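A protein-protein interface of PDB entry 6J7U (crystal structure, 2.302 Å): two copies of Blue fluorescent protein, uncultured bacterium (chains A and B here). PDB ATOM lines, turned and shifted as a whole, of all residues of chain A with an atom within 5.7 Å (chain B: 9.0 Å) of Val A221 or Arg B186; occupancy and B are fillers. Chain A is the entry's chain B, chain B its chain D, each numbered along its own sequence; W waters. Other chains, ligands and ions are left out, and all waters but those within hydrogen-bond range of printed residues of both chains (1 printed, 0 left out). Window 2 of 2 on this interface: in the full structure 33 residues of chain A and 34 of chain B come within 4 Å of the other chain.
NH2 of Arg B186 sits at hydrogen-bond distance from O of Ala A261 (3.1 Å). The backbone carbonyl oxygen (O) of Gly A258 sits at hydrogen-bond distance from the guanidinium group (NH2) of Arg B186, 3.2 Å away. The guanidinium group (NH2) of Arg B186 lies within hydrogen-bond range of the backbone carbonyl oxygen (O) of Phe A259. The backbone carbonyl oxygen (O) of Val A221 lies within hydrogen-bond range of the guanidinium group (NH1) of Arg B186, at 3.0 Å.
OG1 of Thr B249 lies within hydrogen-bond range of N of Ala B195, 2.9 Å away. The backbone carbonyl oxygen of Gly A258 lies within hydrogen-bond range of the side-chain hydroxyl of Ser A223 (3.0 Å).
O of Leu A222 touches NH1 of Arg B186, 3.5 Å away. Leu A222 touches Tyr B247. O of Ala B185 touches CB of Ser A223, at 3.5 Å. Ser A223 touches Arg B186. Gly B189 touches Ser A223. O of Ser A223 touches N of Ala B190 (3.8 Å). Thr B249 touches Gly A258 (CG2 to N, 3.3 Å). Ala A261 touches Arg B182.
No residue of chain B comes within 4 Å of Ala A220. Val A221 touches just one residue of chain B: Arg B186. Of the printed residues of chain B, Leu A222 touches Arg B186 and Tyr B247. Of chain B, only Arg B182 and Arg B186 come within 4 Å of Ala A261. Of the printed residues of chain A, Arg B182 touches Ala A261. Leu B184 touches none of the printed residues of chain A. Of the printed residues of chain A, Ala B185 touches Ser A223. Arg B186 touches six residues of chain A. Of the printed residues of chain A, Ala B190 touches Ser A223. Of the printed residues of chain A, Thr B249 touches Gly A258 (3.3 Å). The nearest residue of chain A that does not touch Arg B186 is Ala A260 (4.4 Å).
Printed residues of chain A that touch a printed residue of chain B: Val A221, Leu A222, Ser A223, Gly A258, Phe A259 and Ala A261. Hydrophobic or aromatic side chains of chain A that line the printed part of chain B: Leu A222 and Ala A261. Of the 20 printed residues of chain B, 7 touch a printed residue of chain A. Among the printed residues, no Asp or Glu carboxylate lies within 4 Å of a Lys or Arg side-chain nitrogen of the other chain.
No position is printed for both chains. Of the 12 pairs that touch across the chains among the printed residues, none has its exchanged pair printed and touching as well.
Water W1 lies within hydrogen-bond range of NH1 of Arg B186 (2.7 Å) and O of Leu A222 (3.1 Å).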
ATOM      1  N   GLU A 217      -7.203 -19.881  34.600  1.00  0.00           N
ATOM      2  CA  GLU A 217      -7.289 -20.727  33.410  1.00  0.00           C
ATOM      3  C   GLU A 217      -6.566 -20.090  32.237  1.00  0.00           C
ATOM      4  O   GLU A 217      -6.112 -20.796  31.331  1.00  0.00           O
ATOM      5  CB  GLU A 217      -8.753 -21.010  33.031  1.00  0.00           C
ATOM      6  CG  GLU A 217      -9.512 -19.829  32.416  1.00  0.00           C
ATOM      7  CD  GLU A 217     -11.018 -20.098  32.212  1.00  0.00           C
ATOM      8  OE1 GLU A 217     -11.826 -19.820  33.133  1.00  0.00           O
ATOM      9  OE2 GLU A 217     -11.395 -20.581  31.120  1.00  0.00           O
ATOM     10  N   LEU A 218      -6.439 -18.766  32.250  1.00  0.00           N
ATOM     11  CA  LEU A 218      -5.710 -18.076  31.200  1.00  0.00           C
ATOM     12  C   LEU A 218      -4.204 -18.261  31.341  1.00  0.00           C
ATOM     13  O   LEU A 218      -3.514 -18.509  30.345  1.00  0.00           O
ATOM     14  CB  LEU A 218      -6.069 -16.601  31.212  1.00  0.00           C
ATOM     15  CG  LEU A 218      -5.434 -15.813  30.095  1.00  0.00           C
ATOM     16  CD1 LEU A 218      -5.709 -16.472  28.765  1.00  0.00           C
ATOM     17  CD2 LEU A 218      -6.062 -14.449  30.184  1.00  0.00           C
ATOM     18  N   VAL A 219      -3.677 -18.186  32.571  1.00  0.00           N
ATOM     19  CA  VAL A 219      -2.238 -18.410  32.757  1.00  0.00           C
ATOM     20  C   VAL A 219      -1.859 -19.789  32.260  1.00  0.00           C
ATOM     21  O   VAL A 219      -0.805 -19.967  31.645  1.00  0.00           O
ATOM     22  CB  VAL A 219      -1.827 -18.213  34.233  1.00  0.00           C
ATOM     23  CG1 VAL A 219      -0.466 -18.793  34.484  1.00  0.00           C
ATOM     24  CG2 VAL A 219      -1.799 -16.731  34.569  1.00  0.00           C
ATOM     25  N   ALA A 220      -2.788 -20.736  32.363  1.00  0.00           N
ATOM     26  CA  ALA A 220      -2.514 -22.125  32.046  1.00  0.00           C
ATOM     27  C   ALA A 220      -2.139 -22.326  30.586  1.00  0.00           C
ATOM     28  O   ALA A 220      -1.610 -23.388  30.240  1.00  0.00           O
ATOM     29  CB  ALA A 220      -3.731 -22.968  32.410  1.00  0.00           C
ATOM     30  N   VAL A 221      -2.508 -21.388  29.707  1.00  0.00           N
ATOM     31  CA  VAL A 221      -2.212 -21.478  28.282  1.00  0.00           C
ATOM     32  C   VAL A 221      -1.066 -20.556  27.840  1.00  0.00           C
ATOM     33  O   VAL A 221      -0.817 -20.436  26.636  1.00  0.00           O
ATOM     34  CB  VAL A 221      -3.497 -21.242  27.453  1.00  0.00           C
ATOM     35  CG1 VAL A 221      -4.570 -22.249  27.863  1.00  0.00           C
ATOM     36  CG2 VAL A 221      -4.037 -19.817  27.639  1.00  0.00           C
ATOM     37  N   LEU A 222      -0.385 -19.880  28.761  1.00  0.00           N
ATOM     38  CA  LEU A 222       0.723 -19.007  28.379  1.00  0.00           C
ATOM     39  C   LEU A 222       2.035 -19.803  28.322  1.00  0.00           C
ATOM     40  O   LEU A 222       2.130 -20.903  28.858  1.00  0.00           O
ATOM     41  CB  LEU A 222       0.836 -17.813  29.340  1.00  0.00           C
ATOM     42  CG  LEU A 222      -0.327 -16.804  29.391  1.00  0.00           C
ATOM     43  CD1 LEU A 222      -0.085 -15.644  30.409  1.00  0.00           C
ATOM     44  CD2 LEU A 222      -0.681 -16.274  27.977  1.00  0.00           C
ATOM     45  N   SER A 223       3.035 -19.266  27.605  1.00  0.00           N
ATOM     46  CA  SER A 223       4.374 -19.874  27.659  1.00  0.00           C
ATOM     47  C   SER A 223       5.130 -19.472  28.924  1.00  0.00           C
ATOM     48  O   SER A 223       5.818 -20.301  29.536  1.00  0.00           O
ATOM     49  CB  SER A 223       5.175 -19.527  26.408  1.00  0.00           C
ATOM     50  OG  SER A 223       4.538 -20.092  25.262  1.00  0.00           O
ATOM     51  N   GLY A 258       3.848 -15.412  25.180  1.00  0.00           N
ATOM     52  CA  GLY A 258       3.752 -16.694  24.503  1.00  0.00           C
ATOM     53  C   GLY A 258       2.354 -17.276  24.376  1.00  0.00           C
ATOM     54  O   GLY A 258       2.221 -18.485  24.178  1.00  0.00           O
ATOM     55  N   PHE A 259       1.298 -16.452  24.492  1.00  0.00           N
ATOM     56  CA  PHE A 259      -0.069 -16.943  24.327  1.00  0.00           C
ATOM     57  C   PHE A 259      -0.253 -17.559  22.949  1.00  0.00           C
ATOM     58  O   PHE A 259      -0.895 -18.611  22.801  1.00  0.00           O
ATOM     59  CB  PHE A 259      -1.054 -15.777  24.546  1.00  0.00           C
ATOM     60  CG  PHE A 259      -2.514 -16.059  24.134  1.00  0.00           C
ATOM     61  CD1 PHE A 259      -2.936 -15.890  22.813  1.00  0.00           C
ATOM     62  CD2 PHE A 259      -3.482 -16.360  25.092  1.00  0.00           C
ATOM     63  CE1 PHE A 259      -4.257 -16.102  22.460  1.00  0.00           C
ATOM     64  CE2 PHE A 259      -4.832 -16.573  24.720  1.00  0.00           C
ATOM     65  CZ  PHE A 259      -5.198 -16.445  23.413  1.00  0.00           C
ATOM     66  N   ALA A 260       0.361 -16.956  21.935  1.00  0.00           N
ATOM     67  CA  ALA A 260       0.152 -17.422  20.570  1.00  0.00           C
ATOM     68  C   ALA A 260       1.091 -18.541  20.153  1.00  0.00           C
ATOM     69  O   ALA A 260       0.832 -19.165  19.128  1.00  0.00           O
ATOM     70  CB  ALA A 260       0.331 -16.273  19.577  1.00  0.00           C
ATOM     71  N   ALA A 261       2.132 -18.846  20.935  1.00  0.00           N
ATOM     72  CA  ALA A 261       3.252 -19.661  20.451  1.00  0.00           C
ATOM     73  C   ALA A 261       2.826 -21.058  20.018  1.00  0.00           C
ATOM     74  O   ALA A 261       2.243 -21.772  20.841  1.00  0.00           O
ATOM     75  CB  ALA A 261       4.386 -19.747  21.544  1.00  0.00           C
ATOM     76  N   GLY B 179       8.507 -22.468  13.480  1.00  0.00           N
ATOM     77  CA  GLY B 179       8.099 -23.535  14.379  1.00  0.00           C
ATOM     78  C   GLY B 179       9.171 -23.846  15.403  1.00  0.00           C
ATOM     79  O   GLY B 179       8.882 -24.120  16.566  1.00  0.00           O
ATOM     80  N   MET B 180      10.429 -23.772  15.010  1.00  0.00           N
ATOM     81  CA  MET B 180      11.417 -24.023  16.041  1.00  0.00           C
ATOM     82  C   MET B 180      11.269 -23.005  17.164  1.00  0.00           C
ATOM     83  O   MET B 180      11.276 -23.364  18.348  1.00  0.00           O
ATOM     84  CB  MET B 180      12.840 -23.981  15.459  1.00  0.00           C
ATOM     85  CG  MET B 180      13.922 -24.441  16.443  1.00  0.00           C
ATOM     86  SD  MET B 180      15.575 -23.975  15.876  1.00  0.00           S
ATOM     87  CE  MET B 180      15.638 -24.674  14.211  1.00  0.00           C
ATOM     88  N   THR B 181      11.042 -21.740  16.820  1.00  0.00           N
ATOM     89  CA  THR B 181      11.032 -20.723  17.867  1.00  0.00           C
ATOM     90  C   THR B 181       9.809 -20.856  18.766  1.00  0.00           C
ATOM     91  O   THR B 181       9.925 -20.770  20.005  1.00  0.00           O
ATOM     92  CB  THR B 181      11.135 -19.341  17.245  1.00  0.00           C
ATOM     93  OG1 THR B 181      12.296 -19.311  16.424  1.00  0.00           O
ATOM     94  CG2 THR B 181      11.320 -18.330  18.311  1.00  0.00           C
ATOM     95  N   ARG B 182       8.632 -21.113  18.163  1.00  0.00           N
ATOM     96  CA  ARG B 182       7.418 -21.257  18.960  1.00  0.00           C
ATOM     97  C   ARG B 182       7.501 -22.459  19.882  1.00  0.00           C
ATOM     98  O   ARG B 182       7.059 -22.399  21.033  1.00  0.00           O
ATOM     99  CB  ARG B 182       6.198 -21.334  18.047  1.00  0.00           C
ATOM    100  CG  ARG B 182       5.839 -19.999  17.410  1.00  0.00           C
ATOM    101  CD  ARG B 182       4.499 -20.046  16.639  1.00  0.00           C
ATOM    102  NE  ARG B 182       4.616 -20.759  15.353  1.00  0.00           N
ATOM    103  CZ  ARG B 182       4.891 -20.225  14.142  1.00  0.00           C
ATOM    104  NH1 ARG B 182       5.083 -18.912  14.007  1.00  0.00           N
ATOM    105  NH2 ARG B 182       4.974 -21.020  13.057  1.00  0.00           N
ATOM    106  N   GLY B 183       8.075 -23.563  19.414  1.00  0.00           N
ATOM    107  CA  GLY B 183       8.205 -24.709  20.296  1.00  0.00           C
ATOM    108  C   GLY B 183       9.218 -24.452  21.394  1.00  0.00           C
ATOM    109  O   GLY B 183       9.005 -24.828  22.560  1.00  0.00           O
ATOM    110  N   LEU B 184      10.310 -23.756  21.056  1.00  0.00           N
ATOM    111  CA  LEU B 184      11.269 -23.450  22.101  1.00  0.00           C
ATOM    112  C   LEU B 184      10.616 -22.602  23.173  1.00  0.00           C
ATOM    113  O   LEU B 184      10.816 -22.839  24.374  1.00  0.00           O
ATOM    114  CB  LEU B 184      12.487 -22.732  21.512  1.00  0.00           C
ATOM    115  CG  LEU B 184      13.499 -23.545  20.669  1.00  0.00           C
ATOM    116  CD1 LEU B 184      14.479 -22.606  19.913  1.00  0.00           C
ATOM    117  CD2 LEU B 184      14.267 -24.561  21.499  1.00  0.00           C
ATOM    118  N   ALA B 185       9.752 -21.664  22.760  1.00  0.00           N
ATOM    119  CA  ALA B 185       9.116 -20.783  23.730  1.00  0.00           C
ATOM    120  C   ALA B 185       8.271 -21.561  24.719  1.00  0.00           C
ATOM    121  O   ALA B 185       8.192 -21.183  25.899  1.00  0.00           O
ATOM    122  CB  ALA B 185       8.264 -19.750  23.016  1.00  0.00           C
ATOM    123  N   ARG B 186       7.627 -22.644  24.264  1.00  0.00           N
ATOM    124  CA  ARG B 186       6.885 -23.523  25.175  1.00  0.00           C
ATOM    125  C   ARG B 186       7.829 -24.373  26.011  1.00  0.00           C
ATOM    126  O   ARG B 186       7.585 -24.613  27.196  1.00  0.00           O
ATOM    127  CB  ARG B 186       5.951 -24.455  24.394  1.00  0.00           C
ATOM    128  CG  ARG B 186       4.842 -23.802  23.640  1.00  0.00           C
ATOM    129  CD  ARG B 186       3.665 -23.477  24.535  1.00  0.00           C
ATOM    130  NE  ARG B 186       2.691 -22.689  23.775  1.00  0.00           N
ATOM    131  CZ  ARG B 186       1.654 -22.059  24.322  1.00  0.00           C
ATOM    132  NH1 ARG B 186       1.470 -22.132  25.639  1.00  0.00           N
ATOM    133  NH2 ARG B 186       0.835 -21.325  23.560  1.00  0.00           N
ATOM    134  N   ASP B 187       8.888 -24.874  25.391  1.00  0.00           N
ATOM    135  CA  ASP B 187       9.779 -25.777  26.087  1.00  0.00           C
ATOM    136  C   ASP B 187      10.430 -25.079  27.260  1.00  0.00           C
ATOM    137  O   ASP B 187      10.604 -25.677  28.328  1.00  0.00           O
ATOM    138  CB  ASP B 187      10.853 -26.266  25.121  1.00  0.00           C
ATOM    139  CG  ASP B 187      10.401 -27.427  24.255  1.00  0.00           C
ATOM    140  OD1 ASP B 187       9.509 -28.195  24.667  1.00  0.00           O
ATOM    141  OD2 ASP B 187      10.936 -27.583  23.132  1.00  0.00           O
ATOM    142  N   LEU B 188      10.750 -23.793  27.100  1.00  0.00           N
ATOM    143  CA  LEU B 188      11.609 -23.088  28.040  1.00  0.00           C
ATOM    144  C   LEU B 188      10.886 -22.018  28.852  1.00  0.00           C
ATOM    145  O   LEU B 188      11.481 -21.458  29.775  1.00  0.00           O
ATOM    146  CB  LEU B 188      12.806 -22.481  27.278  1.00  0.00           C
ATOM    147  CG  LEU B 188      13.617 -23.553  26.530  1.00  0.00           C
ATOM    148  CD1 LEU B 188      14.584 -22.990  25.526  1.00  0.00           C
ATOM    149  CD2 LEU B 188      14.347 -24.384  27.579  1.00  0.00           C
ATOM    150  N   GLY B 189       9.591 -21.787  28.604  1.00  0.00           N
ATOM    151  CA  GLY B 189       8.913 -20.655  29.217  1.00  0.00           C
ATOM    152  C   GLY B 189       8.804 -20.753  30.716  1.00  0.00           C
ATOM    153  O   GLY B 189       8.805 -19.729  31.406  1.00  0.00           O
ATOM    154  N   ALA B 190       8.753 -21.976  31.241  1.00  0.00           N
ATOM    155  CA  ALA B 190       8.716 -22.195  32.675  1.00  0.00           C
ATOM    156  C   ALA B 190       9.977 -21.707  33.378  1.00  0.00           C
ATOM    157  O   ALA B 190       9.923 -21.441  34.582  1.00  0.00           O
ATOM    158  CB  ALA B 190       8.521 -23.681  32.967  1.00  0.00           C
ATOM    159  N   ARG B 191      11.115 -21.604  32.680  1.00  0.00           N
ATOM    160  CA  ARG B 191      12.332 -21.047  33.269  1.00  0.00           C
ATOM    161  C   ARG B 191      12.451 -19.549  33.043  1.00  0.00           C
ATOM    162  O   ARG B 191      13.499 -18.957  33.375  1.00  0.00           O
ATOM    163  CB  ARG B 191      13.564 -21.759  32.707  1.00  0.00           C
ATOM    164  CG  ARG B 191      13.629 -23.183  33.191  1.00  0.00           C
ATOM    165  CD  ARG B 191      14.446 -24.054  32.261  1.00  0.00           C
ATOM    166  NE  ARG B 191      15.842 -23.619  32.198  1.00  0.00           N
ATOM    167  CZ  ARG B 191      16.760 -24.147  31.400  1.00  0.00           C
ATOM    168  NH1 ARG B 191      16.446 -25.145  30.579  1.00  0.00           N
ATOM    169  NH2 ARG B 191      17.993 -23.670  31.438  1.00  0.00           N
ATOM    170  N   GLY B 192      11.430 -18.926  32.443  1.00  0.00           N
ATOM    171  CA  GLY B 192      11.464 -17.512  32.167  1.00  0.00           C
ATOM    172  C   GLY B 192      12.197 -17.174  30.902  1.00  0.00           C
ATOM    173  O   GLY B 192      12.308 -15.984  30.558  1.00  0.00           O
ATOM    174  N   ILE B 193      12.716 -18.190  30.210  1.00  0.00           N
ATOM    175  CA  ILE B 193      13.425 -17.978  28.961  1.00  0.00           C
ATOM    176  C   ILE B 193      12.456 -17.662  27.835  1.00  0.00           C
ATOM    177  O   ILE B 193      11.479 -18.362  27.625  1.00  0.00           O
ATOM    178  CB  ILE B 193      14.296 -19.215  28.651  1.00  0.00           C
ATOM    179  CG1 ILE B 193      15.459 -19.247  29.658  1.00  0.00           C
ATOM    180  CG2 ILE B 193      14.785 -19.208  27.212  1.00  0.00           C
ATOM    181  CD1 ILE B 193      16.185 -20.563  29.718  1.00  0.00           C
ATOM    182  N   THR B 194      12.803 -16.686  27.032  1.00  0.00           N
ATOM    183  CA  THR B 194      12.027 -16.331  25.872  1.00  0.00           C
ATOM    184  C   THR B 194      12.756 -16.801  24.627  1.00  0.00           C
ATOM    185  O   THR B 194      13.985 -16.887  24.601  1.00  0.00           O
ATOM    186  CB  THR B 194      11.825 -14.813  25.770  1.00  0.00           C
ATOM    187  OG1 THR B 194      13.061 -14.206  25.404  1.00  0.00           O
ATOM    188  CG2 THR B 194      11.380 -14.214  27.114  1.00  0.00           C
ATOM    189  N   ALA B 195      12.002 -17.044  23.571  1.00  0.00           N
ATOM    190  CA  ALA B 195      12.581 -17.388  22.278  1.00  0.00           C
ATOM    191  C   ALA B 195      11.796 -16.657  21.195  1.00  0.00           C
ATOM    192  O   ALA B 195      10.574 -16.855  21.101  1.00  0.00           O
ATOM    193  CB  ALA B 195      12.586 -18.915  22.041  1.00  0.00           C
ATOM    194  N   TYR B 247       8.636 -10.049  28.508  1.00  0.00           N
ATOM    195  CA  TYR B 247       7.339 -10.684  28.266  1.00  0.00           C
ATOM    196  C   TYR B 247       7.083 -10.991  26.795  1.00  0.00           C
ATOM    197  O   TYR B 247       5.957 -11.348  26.461  1.00  0.00           O
ATOM    198  CB  TYR B 247       6.177  -9.820  28.786  1.00  0.00           C
ATOM    199  CG  TYR B 247       4.884 -10.584  29.119  1.00  0.00           C
ATOM    200  CD1 TYR B 247       4.867 -11.557  30.125  1.00  0.00           C
ATOM    201  CD2 TYR B 247       3.679 -10.315  28.456  1.00  0.00           C
ATOM    202  CE1 TYR B 247       3.711 -12.238  30.456  1.00  0.00           C
ATOM    203  CE2 TYR B 247       2.504 -11.018  28.787  1.00  0.00           C
ATOM    204  CZ  TYR B 247       2.546 -11.969  29.793  1.00  0.00           C
ATOM    205  OH  TYR B 247       1.422 -12.698  30.138  1.00  0.00           O
ATOM    206  N   THR B 249       7.776 -13.509  23.841  1.00  0.00           N
ATOM    207  CA  THR B 249       8.325 -14.840  23.580  1.00  0.00           C
ATOM    208  C   THR B 249       7.439 -15.567  22.571  1.00  0.00           C
ATOM    209  O   THR B 249       6.221 -15.361  22.522  1.00  0.00           O
ATOM    210  CB  THR B 249       8.455 -15.665  24.872  1.00  0.00           C
ATOM    211  OG1 THR B 249       9.309 -16.817  24.660  1.00  0.00           O
ATOM    212  CG2 THR B 249       7.039 -16.113  25.389  1.00  0.00           C
ATOM    213  N   GLY B 250       8.080 -16.371  21.727  1.00  0.00           N
ATOM    214  CA  GLY B 250       7.365 -17.076  20.684  1.00  0.00           C
ATOM    215  C   GLY B 250       6.932 -16.220  19.523  1.00  0.00           C
ATOM    216  O   GLY B 250       6.076 -16.639  18.756  1.00  0.00           O
HETATM  217  O   HOH W   1       2.674 -23.642  27.520  1.00  0.00           O
